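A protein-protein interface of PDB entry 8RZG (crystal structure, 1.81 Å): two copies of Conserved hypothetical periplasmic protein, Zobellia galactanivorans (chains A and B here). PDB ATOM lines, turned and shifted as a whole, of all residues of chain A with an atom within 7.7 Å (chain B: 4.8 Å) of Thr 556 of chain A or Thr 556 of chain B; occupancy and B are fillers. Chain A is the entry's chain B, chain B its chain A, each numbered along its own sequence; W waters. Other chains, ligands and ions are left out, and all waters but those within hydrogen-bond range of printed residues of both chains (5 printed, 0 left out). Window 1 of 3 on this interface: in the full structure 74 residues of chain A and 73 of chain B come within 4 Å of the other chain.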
ATOM      1  N   ARG A 179       0.954 -21.274 -12.730  1.00  0.00           N
ATOM      2  CA  ARG A 179       0.423 -20.905 -11.423  1.00  0.00           C
ATOM      3  C   ARG A 179       0.164 -22.139 -10.569  1.00  0.00           C
ATOM      4  O   ARG A 179       0.421 -22.135  -9.359  1.00  0.00           O
ATOM      5  CB  ARG A 179      -0.877 -20.116 -11.596  1.00  0.00           C
ATOM      6  CG  ARG A 179      -0.723 -18.851 -12.438  1.00  0.00           C
ATOM      7  CD  ARG A 179       0.049 -17.785 -11.678  1.00  0.00           C
ATOM      8  NE  ARG A 179       0.093 -16.532 -12.434  1.00  0.00           N
ATOM      9  CZ  ARG A 179       0.737 -15.442 -12.032  1.00  0.00           C
ATOM     10  NH1 ARG A 179       1.381 -15.436 -10.871  1.00  0.00           N
ATOM     11  NH2 ARG A 179       0.732 -14.353 -12.790  1.00  0.00           N
ATOM     12  N   LYS A 182       3.408 -23.617  -8.926  1.00  0.00           N
ATOM     13  CA  LYS A 182       3.861 -22.790  -7.808  1.00  0.00           C
ATOM     14  C   LYS A 182       2.905 -22.905  -6.623  1.00  0.00           C
ATOM     15  O   LYS A 182       3.337 -22.958  -5.468  1.00  0.00           O
ATOM     16  CB  LYS A 182       3.986 -21.321  -8.234  1.00  0.00           C
ATOM     17  CG  LYS A 182       5.129 -21.001  -9.221  1.00  0.00           C
ATOM     18  CD  LYS A 182       5.202 -19.491  -9.544  1.00  0.00           C
ATOM     19  CE  LYS A 182       4.132 -19.068 -10.549  1.00  0.00           C
ATOM     20  NZ  LYS A 182       4.283 -17.637 -10.979  1.00  0.00           N
ATOM     21  N   TYR A 518      -1.896  -3.971  -2.994  1.00  0.00           N
ATOM     22  CA  TYR A 518      -1.082  -5.180  -2.843  1.00  0.00           C
ATOM     23  C   TYR A 518       0.390  -4.846  -3.030  1.00  0.00           C
ATOM     24  O   TYR A 518       0.737  -4.050  -3.907  1.00  0.00           O
ATOM     25  CB  TYR A 518      -1.510  -6.263  -3.848  1.00  0.00           C
ATOM     26  CG  TYR A 518      -2.921  -6.658  -3.552  1.00  0.00           C
ATOM     27  CD1 TYR A 518      -3.196  -7.593  -2.568  1.00  0.00           C
ATOM     28  CD2 TYR A 518      -3.987  -6.014  -4.173  1.00  0.00           C
ATOM     29  CE1 TYR A 518      -4.516  -7.917  -2.229  1.00  0.00           C
ATOM     30  CE2 TYR A 518      -5.301  -6.322  -3.842  1.00  0.00           C
ATOM     31  CZ  TYR A 518      -5.560  -7.273  -2.875  1.00  0.00           C
ATOM     32  OH  TYR A 518      -6.866  -7.577  -2.557  1.00  0.00           O
ATOM     33  N   LEU A 519       1.245  -5.429  -2.188  1.00  0.00           N
ATOM     34  CA  LEU A 519       2.661  -5.487  -2.520  1.00  0.00           C
ATOM     35  C   LEU A 519       2.862  -6.354  -3.757  1.00  0.00           C
ATOM     36  O   LEU A 519       2.043  -7.219  -4.069  1.00  0.00           O
ATOM     37  CB  LEU A 519       3.484  -6.082  -1.372  1.00  0.00           C
ATOM     38  CG  LEU A 519       3.661  -5.348  -0.057  1.00  0.00           C
ATOM     39  CD1 LEU A 519       4.633  -6.148   0.804  1.00  0.00           C
ATOM     40  CD2 LEU A 519       4.174  -3.922  -0.292  1.00  0.00           C
ATOM     41  N   GLU A 520       3.968  -6.126  -4.469  1.00  0.00           N
ATOM     42  CA  GLU A 520       4.278  -6.975  -5.618  1.00  0.00           C
ATOM     43  C   GLU A 520       4.859  -8.312  -5.178  1.00  0.00           C
ATOM     44  O   GLU A 520       4.425  -9.363  -5.654  1.00  0.00           O
ATOM     45  CB  GLU A 520       5.247  -6.259  -6.562  1.00  0.00           C
ATOM     46  CG  GLU A 520       4.648  -5.026  -7.205  1.00  0.00           C
ATOM     47  CD  GLU A 520       5.713  -4.125  -7.803  1.00  0.00           C
ATOM     48  OE1 GLU A 520       6.414  -4.579  -8.725  1.00  0.00           O
ATOM     49  OE2 GLU A 520       5.865  -2.986  -7.312  1.00  0.00           O
ATOM     50  N   GLN A 549       4.227   2.896  -6.463  1.00  0.00           N
ATOM     51  CA  GLN A 549       5.265   1.948  -6.865  1.00  0.00           C
ATOM     52  C   GLN A 549       4.758   0.941  -7.896  1.00  0.00           C
ATOM     53  O   GLN A 549       5.550   0.399  -8.676  1.00  0.00           O
ATOM     54  CB  GLN A 549       5.814   1.200  -5.647  1.00  0.00           C
ATOM     55  CG  GLN A 549       6.859   1.976  -4.857  1.00  0.00           C
ATOM     56  CD  GLN A 549       6.251   2.946  -3.858  1.00  0.00           C
ATOM     57  OE1 GLN A 549       5.029   3.080  -3.763  1.00  0.00           O
ATOM     58  NE2 GLN A 549       7.109   3.624  -3.100  1.00  0.00           N
ATOM     59  N   ASP A 550       3.454   0.691  -7.918  1.00  0.00           N
ATOM     60  CA  ASP A 550       2.850  -0.361  -8.736  1.00  0.00           C
ATOM     61  C   ASP A 550       1.650   0.207  -9.483  1.00  0.00           C
ATOM     62  O   ASP A 550       0.524  -0.275  -9.333  1.00  0.00           O
ATOM     63  CB  ASP A 550       2.441  -1.537  -7.840  1.00  0.00           C
ATOM     64  CG  ASP A 550       1.904  -2.738  -8.616  1.00  0.00           C
ATOM     65  OD1 ASP A 550       2.192  -2.861  -9.827  1.00  0.00           O
ATOM     66  OD2 ASP A 550       1.195  -3.577  -7.998  1.00  0.00           O
ATOM     67  N   PRO A 551       1.853   1.248 -10.291  1.00  0.00           N
ATOM     68  CA  PRO A 551       0.720   1.980 -10.858  1.00  0.00           C
ATOM     69  C   PRO A 551       0.087   1.214 -12.011  1.00  0.00           C
ATOM     70  O   PRO A 551       0.583   0.187 -12.476  1.00  0.00           O
ATOM     71  CB  PRO A 551       1.365   3.282 -11.346  1.00  0.00           C
ATOM     72  CG  PRO A 551       2.723   2.828 -11.804  1.00  0.00           C
ATOM     73  CD  PRO A 551       3.142   1.760 -10.804  1.00  0.00           C
ATOM     74  N   ASN A 553      -0.024   1.804 -15.053  1.00  0.00           N
ATOM     75  CA  ASN A 553       0.729   1.846 -16.299  1.00  0.00           C
ATOM     76  C   ASN A 553       1.970   0.958 -16.285  1.00  0.00           C
ATOM     77  O   ASN A 553       2.716   0.945 -17.269  1.00  0.00           O
ATOM     78  CB  ASN A 553       1.146   3.290 -16.609  1.00  0.00           C
ATOM     79  CG  ASN A 553       1.787   3.987 -15.419  1.00  0.00           C
ATOM     80  OD1 ASN A 553       1.104   4.332 -14.454  1.00  0.00           O
ATOM     81  ND2 ASN A 553       3.103   4.224 -15.493  1.00  0.00           N
ATOM     82  N   GLU A 554       2.220   0.227 -15.205  1.00  0.00           N
ATOM     83  CA  GLU A 554       3.387  -0.635 -15.095  1.00  0.00           C
ATOM     84  C   GLU A 554       2.949  -2.092 -15.093  1.00  0.00           C
ATOM     85  O   GLU A 554       1.910  -2.438 -14.520  1.00  0.00           O
ATOM     86  CB  GLU A 554       4.190  -0.326 -13.823  1.00  0.00           C
ATOM     87  CG  GLU A 554       5.120   0.885 -13.943  1.00  0.00           C
ATOM     88  CD  GLU A 554       6.280   0.647 -14.890  1.00  0.00           C
ATOM     89  OE1 GLU A 554       6.987  -0.373 -14.725  1.00  0.00           O
ATOM     90  OE2 GLU A 554       6.490   1.479 -15.804  1.00  0.00           O
ATOM     91  N   VAL A 555       3.734  -2.940 -15.739  1.00  0.00           N
ATOM     92  CA  VAL A 555       3.455  -4.373 -15.773  1.00  0.00           C
ATOM     93  C   VAL A 555       4.231  -5.035 -14.641  1.00  0.00           C
ATOM     94  O   VAL A 555       5.463  -4.999 -14.631  1.00  0.00           O
ATOM     95  CB  VAL A 555       3.842  -4.978 -17.129  1.00  0.00           C
ATOM     96  CG1 VAL A 555       3.507  -6.469 -17.156  1.00  0.00           C
ATOM     97  CG2 VAL A 555       3.141  -4.214 -18.267  1.00  0.00           C
ATOM     98  N   THR A 556       3.520  -5.636 -13.686  1.00  0.00           N
ATOM     99  CA  THR A 556       4.166  -6.192 -12.500  1.00  0.00           C
ATOM    100  C   THR A 556       3.538  -7.531 -12.140  1.00  0.00           C
ATOM    101  O   THR A 556       2.633  -8.027 -12.822  1.00  0.00           O
ATOM    102  CB  THR A 556       4.047  -5.264 -11.286  1.00  0.00           C
ATOM    103  OG1 THR A 556       2.676  -5.213 -10.854  1.00  0.00           O
ATOM    104  CG2 THR A 556       4.560  -3.857 -11.588  1.00  0.00           C
ATOM    105  N   ALA A 557       4.005  -8.091 -11.014  1.00  0.00           N
ATOM    106  CA  ALA A 557       3.384  -9.290 -10.470  1.00  0.00           C
ATOM    107  C   ALA A 557       1.877  -9.128 -10.269  1.00  0.00           C
ATOM    108  O   ALA A 557       1.152 -10.125 -10.302  1.00  0.00           O
ATOM    109  CB  ALA A 557       4.064  -9.669  -9.144  1.00  0.00           C
ATOM    110  N   ASN A 558       1.382  -7.902 -10.089  1.00  0.00           N
ATOM    111  CA  ASN A 558      -0.042  -7.679  -9.871  1.00  0.00           C
ATOM    112  C   ASN A 558      -0.810  -7.374 -11.149  1.00  0.00           C
ATOM    113  O   ASN A 558      -2.016  -7.124 -11.080  1.00  0.00           O
ATOM    114  CB  ASN A 558      -0.258  -6.554  -8.854  1.00  0.00           C
ATOM    115  CG  ASN A 558       0.218  -6.939  -7.473  1.00  0.00           C
ATOM    116  OD1 ASN A 558       0.080  -8.097  -7.062  1.00  0.00           O
ATOM    117  ND2 ASN A 558       0.802  -5.982  -6.755  1.00  0.00           N
ATOM    118  N   GLY A 559      -0.165  -7.396 -12.305  1.00  0.00           N
ATOM    119  CA  GLY A 559      -0.867  -7.408 -13.570  1.00  0.00           C
ATOM    120  C   GLY A 559      -0.431  -6.279 -14.483  1.00  0.00           C
ATOM    121  O   GLY A 559       0.412  -5.446 -14.143  1.00  0.00           O
ATOM    122  N   ASP A 560      -1.013  -6.293 -15.682  1.00  0.00           N
ATOM    123  CA  ASP A 560      -0.848  -5.250 -16.678  1.00  0.00           C
ATOM    124  C   ASP A 560      -2.024  -4.278 -16.570  1.00  0.00           C
ATOM    125  O   ASP A 560      -2.787  -4.294 -15.594  1.00  0.00           O
ATOM    126  CB  ASP A 560      -0.697  -5.877 -18.075  1.00  0.00           C
ATOM    127  CG  ASP A 560      -1.886  -6.755 -18.478  1.00  0.00           C
ATOM    128  OD1 ASP A 560      -2.852  -6.868 -17.702  1.00  0.00           O
ATOM    129  OD2 ASP A 560      -1.838  -7.346 -19.575  1.00  0.00           O
ATOM    130  N   PHE A 561      -2.191  -3.413 -17.568  1.00  0.00           N
ATOM    131  CA  PHE A 561      -3.300  -2.470 -17.484  1.00  0.00           C
ATOM    132  C   PHE A 561      -4.645  -3.185 -17.596  1.00  0.00           C
ATOM    133  O   PHE A 561      -5.611  -2.792 -16.934  1.00  0.00           O
ATOM    134  CB  PHE A 561      -3.187  -1.384 -18.555  1.00  0.00           C
ATOM    135  CG  PHE A 561      -4.291  -0.368 -18.475  1.00  0.00           C
ATOM    136  CD1 PHE A 561      -4.214   0.684 -17.585  1.00  0.00           C
ATOM    137  CD2 PHE A 561      -5.433  -0.501 -19.252  1.00  0.00           C
ATOM    138  CE1 PHE A 561      -5.235   1.600 -17.489  1.00  0.00           C
ATOM    139  CE2 PHE A 561      -6.452   0.403 -19.160  1.00  0.00           C
ATOM    140  CZ  PHE A 561      -6.357   1.462 -18.277  1.00  0.00           C
ATOM    141  N   ILE A 563      -5.564  -6.150 -16.470  1.00  0.00           N
ATOM    142  CA  ILE A 563      -5.925  -6.777 -15.207  1.00  0.00           C
ATOM    143  C   ILE A 563      -6.191  -5.724 -14.142  1.00  0.00           C
ATOM    144  O   ILE A 563      -7.153  -5.835 -13.372  1.00  0.00           O
ATOM    145  CB  ILE A 563      -4.813  -7.754 -14.777  1.00  0.00           C
ATOM    146  CG1 ILE A 563      -4.701  -8.911 -15.780  1.00  0.00           C
ATOM    147  CG2 ILE A 563      -5.061  -8.245 -13.364  1.00  0.00           C
ATOM    148  CD1 ILE A 563      -3.402  -9.713 -15.668  1.00  0.00           C
ATOM    149  N   LYS A 564      -5.334  -4.692 -14.061  1.00  0.00           N
ATOM    150  CA  LYS A 564      -5.488  -3.701 -13.000  1.00  0.00           C
ATOM    151  C   LYS A 564      -6.742  -2.863 -13.198  1.00  0.00           C
ATOM    152  O   LYS A 564      -7.424  -2.522 -12.224  1.00  0.00           O
ATOM    153  CB  LYS A 564      -4.247  -2.806 -12.919  1.00  0.00           C
ATOM    154  CG  LYS A 564      -3.069  -3.487 -12.219  1.00  0.00           C
ATOM    155  CD  LYS A 564      -1.757  -2.745 -12.459  1.00  0.00           C
ATOM    156  CE  LYS A 564      -0.640  -3.321 -11.574  1.00  0.00           C
ATOM    157  NZ  LYS A 564       0.679  -2.689 -11.905  1.00  0.00           N
ATOM    158  N   ARG A 567      -9.700  -5.144 -12.179  1.00  0.00           N
ATOM    159  CA  ARG A 567      -9.715  -5.257 -10.724  1.00  0.00           C
ATOM    160  C   ARG A 567     -10.106  -3.940 -10.060  1.00  0.00           C
ATOM    161  O   ARG A 567     -10.785  -3.957  -9.028  1.00  0.00           O
ATOM    162  CB  ARG A 567      -8.350  -5.735 -10.193  1.00  0.00           C
ATOM    163  CG  ARG A 567      -8.410  -6.209  -8.735  1.00  0.00           C
ATOM    164  CD  ARG A 567      -7.039  -6.522  -8.124  1.00  0.00           C
ATOM    165  NE  ARG A 567      -6.314  -7.588  -8.820  1.00  0.00           N
ATOM    166  CZ  ARG A 567      -5.161  -7.423  -9.467  1.00  0.00           C
ATOM    167  NH1 ARG A 567      -4.569  -6.230  -9.523  1.00  0.00           N
ATOM    168  NH2 ARG A 567      -4.585  -8.461 -10.058  1.00  0.00           N
ATOM    169  N   ARG B 179       9.272   2.534 -10.546  1.00  0.00           N
ATOM    170  CA  ARG B 179      10.537   1.807 -10.554  1.00  0.00           C
ATOM    171  C   ARG B 179      11.637   2.608  -9.869  1.00  0.00           C
ATOM    172  O   ARG B 179      12.438   2.051  -9.108  1.00  0.00           O
ATOM    173  CB  ARG B 179      10.945   1.493 -11.993  1.00  0.00           C
ATOM    174  CG  ARG B 179       9.904   0.727 -12.783  1.00  0.00           C
ATOM    175  CD  ARG B 179       9.832  -0.716 -12.315  1.00  0.00           C
ATOM    176  NE  ARG B 179       8.873  -1.482 -13.106  1.00  0.00           N
ATOM    177  CZ  ARG B 179       8.539  -2.746 -12.867  1.00  0.00           C
ATOM    178  NH1 ARG B 179       9.107  -3.418 -11.864  1.00  0.00           N
ATOM    179  NH2 ARG B 179       7.648  -3.346 -13.647  1.00  0.00           N
ATOM    180  N   GLU B 520      10.773 -14.846 -10.818  1.00  0.00           N
ATOM    181  CA  GLU B 520       9.916 -13.671 -10.689  1.00  0.00           C
ATOM    182  C   GLU B 520      10.301 -12.828  -9.474  1.00  0.00           C
ATOM    183  O   GLU B 520      10.521 -11.621  -9.599  1.00  0.00           O
ATOM    184  CB  GLU B 520       8.445 -14.095 -10.611  1.00  0.00           C
ATOM    185  CG  GLU B 520       7.939 -14.795 -11.853  1.00  0.00           C
ATOM    186  CD  GLU B 520       6.661 -15.568 -11.559  1.00  0.00           C
ATOM    187  OE1 GLU B 520       5.692 -14.927 -11.107  1.00  0.00           O
ATOM    188  OE2 GLU B 520       6.653 -16.810 -11.728  1.00  0.00           O
ATOM    189  N   ASP B 550       6.659 -19.332 -15.419  1.00  0.00           N
ATOM    190  CA  ASP B 550       6.584 -17.921 -15.801  1.00  0.00           C
ATOM    191  C   ASP B 550       6.508 -17.834 -17.322  1.00  0.00           C
ATOM    192  O   ASP B 550       7.387 -17.264 -17.975  1.00  0.00           O
ATOM    193  CB  ASP B 550       7.803 -17.177 -15.243  1.00  0.00           C
ATOM    194  CG  ASP B 550       7.758 -15.683 -15.505  1.00  0.00           C
ATOM    195  OD1 ASP B 550       6.663 -15.169 -15.791  1.00  0.00           O
ATOM    196  OD2 ASP B 550       8.824 -15.025 -15.430  1.00  0.00           O
ATOM    197  N   GLU B 554       1.586 -15.678 -19.345  1.00  0.00           N
ATOM    198  CA  GLU B 554       1.237 -15.201 -18.013  1.00  0.00           C
ATOM    199  C   GLU B 554       1.856 -13.829 -17.767  1.00  0.00           C
ATOM    200  O   GLU B 554       2.982 -13.562 -18.194  1.00  0.00           O
ATOM    201  CB  GLU B 554       1.711 -16.184 -16.929  1.00  0.00           C
ATOM    202  CG  GLU B 554       0.801 -17.395 -16.747  1.00  0.00           C
ATOM    203  CD  GLU B 554      -0.550 -17.020 -16.186  1.00  0.00           C
ATOM    204  OE1 GLU B 554      -0.585 -16.330 -15.148  1.00  0.00           O
ATOM    205  OE2 GLU B 554      -1.575 -17.386 -16.803  1.00  0.00           O
ATOM    206  N   VAL B 555       1.109 -12.961 -17.094  1.00  0.00           N
ATOM    207  CA  VAL B 555       1.577 -11.625 -16.738  1.00  0.00           C
ATOM    208  C   VAL B 555       2.172 -11.691 -15.334  1.00  0.00           C
ATOM    209  O   VAL B 555       1.482 -12.024 -14.362  1.00  0.00           O
ATOM    210  CB  VAL B 555       0.444 -10.596 -16.807  1.00  0.00           C
ATOM    211  CG1 VAL B 555       0.986  -9.181 -16.545  1.00  0.00           C
ATOM    212  CG2 VAL B 555      -0.255 -10.669 -18.152  1.00  0.00           C
ATOM    213  N   THR B 556       3.467 -11.414 -15.229  1.00  0.00           N
ATOM    214  CA  THR B 556       4.184 -11.590 -13.977  1.00  0.00           C
ATOM    215  C   THR B 556       5.120 -10.399 -13.773  1.00  0.00           C
ATOM    216  O   THR B 556       5.155  -9.453 -14.573  1.00  0.00           O
ATOM    217  CB  THR B 556       4.969 -12.912 -13.976  1.00  0.00           C
ATOM    218  OG1 THR B 556       6.070 -12.817 -14.892  1.00  0.00           O
ATOM    219  CG2 THR B 556       4.073 -14.108 -14.359  1.00  0.00           C
ATOM    220  N   ALA B 557       5.911 -10.469 -12.704  1.00  0.00           N
ATOM    221  CA  ALA B 557       6.965  -9.488 -12.476  1.00  0.00           C
ATOM    222  C   ALA B 557       7.928  -9.372 -13.656  1.00  0.00           C
ATOM    223  O   ALA B 557       8.540  -8.313 -13.837  1.00  0.00           O
ATOM    224  CB  ALA B 557       7.738  -9.861 -11.197  1.00  0.00           C
ATOM    225  N   ASN B 558       8.082 -10.427 -14.462  1.00  0.00           N
ATOM    226  CA  ASN B 558       8.968 -10.392 -15.620  1.00  0.00           C
ATOM    227  C   ASN B 558       8.279  -9.898 -16.886  1.00  0.00           C
ATOM    228  O   ASN B 558       8.937  -9.773 -17.924  1.00  0.00           O
ATOM    229  CB  ASN B 558       9.597 -11.777 -15.850  1.00  0.00           C
ATOM    230  CG  ASN B 558      10.591 -12.146 -14.749  1.00  0.00           C
ATOM    231  OD1 ASN B 558      11.359 -11.297 -14.289  1.00  0.00           O
ATOM    232  ND2 ASN B 558      10.561 -13.401 -14.310  1.00  0.00           N
ATOM    233  N   GLY B 559       6.985  -9.602 -16.835  1.00  0.00           N
ATOM    234  CA  GLY B 559       6.332  -8.883 -17.912  1.00  0.00           C
ATOM    235  C   GLY B 559       5.108  -9.610 -18.417  1.00  0.00           C
ATOM    236  O   GLY B 559       4.727 -10.670 -17.924  1.00  0.00           O
ATOM    237  N   LYS B 564       7.798  -9.979 -22.918  1.00  0.00           N
ATOM    238  CA  LYS B 564       8.502 -11.257 -22.992  1.00  0.00           C
ATOM    239  C   LYS B 564       8.828 -11.646 -24.434  1.00  0.00           C
ATOM    240  O   LYS B 564       9.886 -12.226 -24.698  1.00  0.00           O
ATOM    241  CB  LYS B 564       7.677 -12.354 -22.302  1.00  0.00           C
ATOM    242  CG  LYS B 564       7.683 -12.255 -20.783  1.00  0.00           C
ATOM    243  CD  LYS B 564       6.647 -13.205 -20.148  1.00  0.00           C
ATOM    244  CE  LYS B 564       6.730 -13.175 -18.636  1.00  0.00           C
ATOM    245  NZ  LYS B 564       5.692 -14.076 -18.016  1.00  0.00           N
HETATM  246  O   HOH W   1       6.611  -0.859 -10.788  1.00  0.00           O
HETATM  247  O   HOH W   2       7.408  -6.310 -16.041  1.00  0.00           O
HETATM  248  O   HOH W   3      -0.533 -10.648 -12.936  1.00  0.00           O
HETATM  249  O   HOH W   4       4.749 -15.716  -8.690  1.00  0.00           O
HETATM  250  O   HOH W   5       9.948  -0.098 -15.985  1.00  0.00           O
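Water W1 lies within hydrogen-bond range of the backbone carbonyl oxygen (O) of Gln 549 of chain A (2.7 Å) and the guanidinium group (NE) of Arg 179 of chain B (3.3 Å). Water W4 lies within hydrogen-bond range of OE1 of Glu 520 of chain B (2.7 Å) and NZ of Lys 182 of chain A (3.0 Å). Water W2 lies within hydrogen-bond range of O of Val 555 of chain A (2.7 Å), O of Ala 557 of chain B (3.2 Å) and N of Gly 559 of chain B (3.4 Å). Water W3 lies within hydrogen-bond range of O of Val 555 of chain B (2.8 Å), O of Ala 557 of chain A (3.2 Å) and N of Gly 559 of chain A (3.3 Å). Water W5 lies within hydrogen-bond range of the side-chain carboxylate of Glu 554 of chain A (3.2 Å) and the guanidinium group of Arg 179 of chain B (3.4 Å).
Asn 553 of chain A touches none of the printed residues of chain B. Thr 556 of chain A touches three residues of chain B. Printed residues of chain B within 4 Å of Asp 560 of chain A: Val 555. Printed residues of chain A within 4 Å of Glu 554 of chain B: Arg 179 (2.8 Å). Thr 556 of chain B touches just these residues of chain A: Arg 179, Thr 556 and Ala 557. The nearest residue of chain B that does not touch Thr 556 of chain A is Val 555 of chain B (4.2 Å). The nearest residue of chain A that does not touch Thr 556 of chain B is Val 555 of chain A (4.3 Å). The nearest printed residue of chain A that does not touch Glu 520 of chain B is Arg 179 of chain A (4.3 Å).
Of the 20 printed residues of chain A, 8 touch a printed residue of chain B. Hydrophobic or aromatic side chains of chain A within 4 Å of the printed part of chain B: Val 555. Among the printed residues, 15 pairs touch across the chains.
NE of Arg 179 of chain B lies within salt-bridge range of OE1 of Glu 554 of chain A, 2.7 Å away. The guanidinium group of Arg 179 of chain B is in hydrogen-bond range of the backbone carbonyl oxygen of Val 555 of chain A, at 2.9 Å. The side-chain amino group of Lys 182 of chain A lies within salt-bridge range of the side-chain carboxylate of Glu 520 of chain B, at 2.6 Å. The side-chain carboxylate (OE1) of Glu 554 of chain B lies within salt-bridge range of the guanidinium group (NE) of Arg 179 of chain A (2.8 Å). The backbone carbonyl oxygen of Val 555 of chain B is in hydrogen-bond range of the guanidinium group of Arg 179 of chain A (2.9 Å). The backbone carbonyl oxygen of Thr 556 of chain B sits close to the backbone carbonyl oxygen of Thr 556 of chain A. N of Ala 557 of chain B lies close to N of Ala 557 of chain A.
The backbone carbonyl oxygen (O) of Glu 554 of chain B lies within hydrogen-bond range of the side-chain amino group (NZ) of Lys 564 of chain B, 2.8 Å away. OG1 of Thr 556 of chain B lies within hydrogen-bond range of NZ of Lys 564 of chain B, 3.4 Å away. OG1 of Thr 556 of chain A is in hydrogen-bond range of OD1 of Asp 550 of chain A (2.6 Å). The side-chain amino group (NZ) of Lys 564 of chain A lies within hydrogen-bond range of the backbone carbonyl oxygen (O) of Glu 554 of chain A (2.9 Å). The backbone NH of Asn 558 of chain A sits close to the side-chain hydroxyl of Thr 556 of chain A, 3.1 Å away. The side-chain carboxylate of Asp 560 of chain A lies within hydrogen-bond range of the backbone NH of Ile 563 of chain A, at 3.1 Å.
Arg 179 of chain A touches Glu 554 of chain B, and with the chains exchanged Glu 554 of chain A touches Arg 179 of chain B. Arg 179 of chain A touches Val 555 of chain B, and with the chains exchanged Val 555 of chain A touches Arg 179 of chain B. Arg 179 of chain A touches Thr 556 of chain B, and with the chains exchanged Thr 556 of chain A touches Arg 179 of chain B. Thr 556 of chain A touches Ala 557 of chain B, and with the chains exchanged Ala 557 of chain A touches Thr 556 of chain B. Of the 15 pairs that touch across the chains among the printed residues, 13 have their exchanged pair printed and touching as well.
NH2 of Arg 179 of chain A touches CG2 of Thr 556 of chain B, at 3.7 Å. Val 555 of chain A touches Val 555 of chain B. Gly 559 of chain B touches Val 555 of chain A. Thr 556 of chain A touches Arg 179 of chain B. Thr 556 of chain A touches Ala 557 of chain B (C to N, 3.8 Å). Ala 557 of chain A touches Thr 556 of chain B. Val 555 of chain B touches Gly 559 of chain A. Asp 560 of chain A touches Val 555 of chain B (N to CG1, 3.6 Å).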
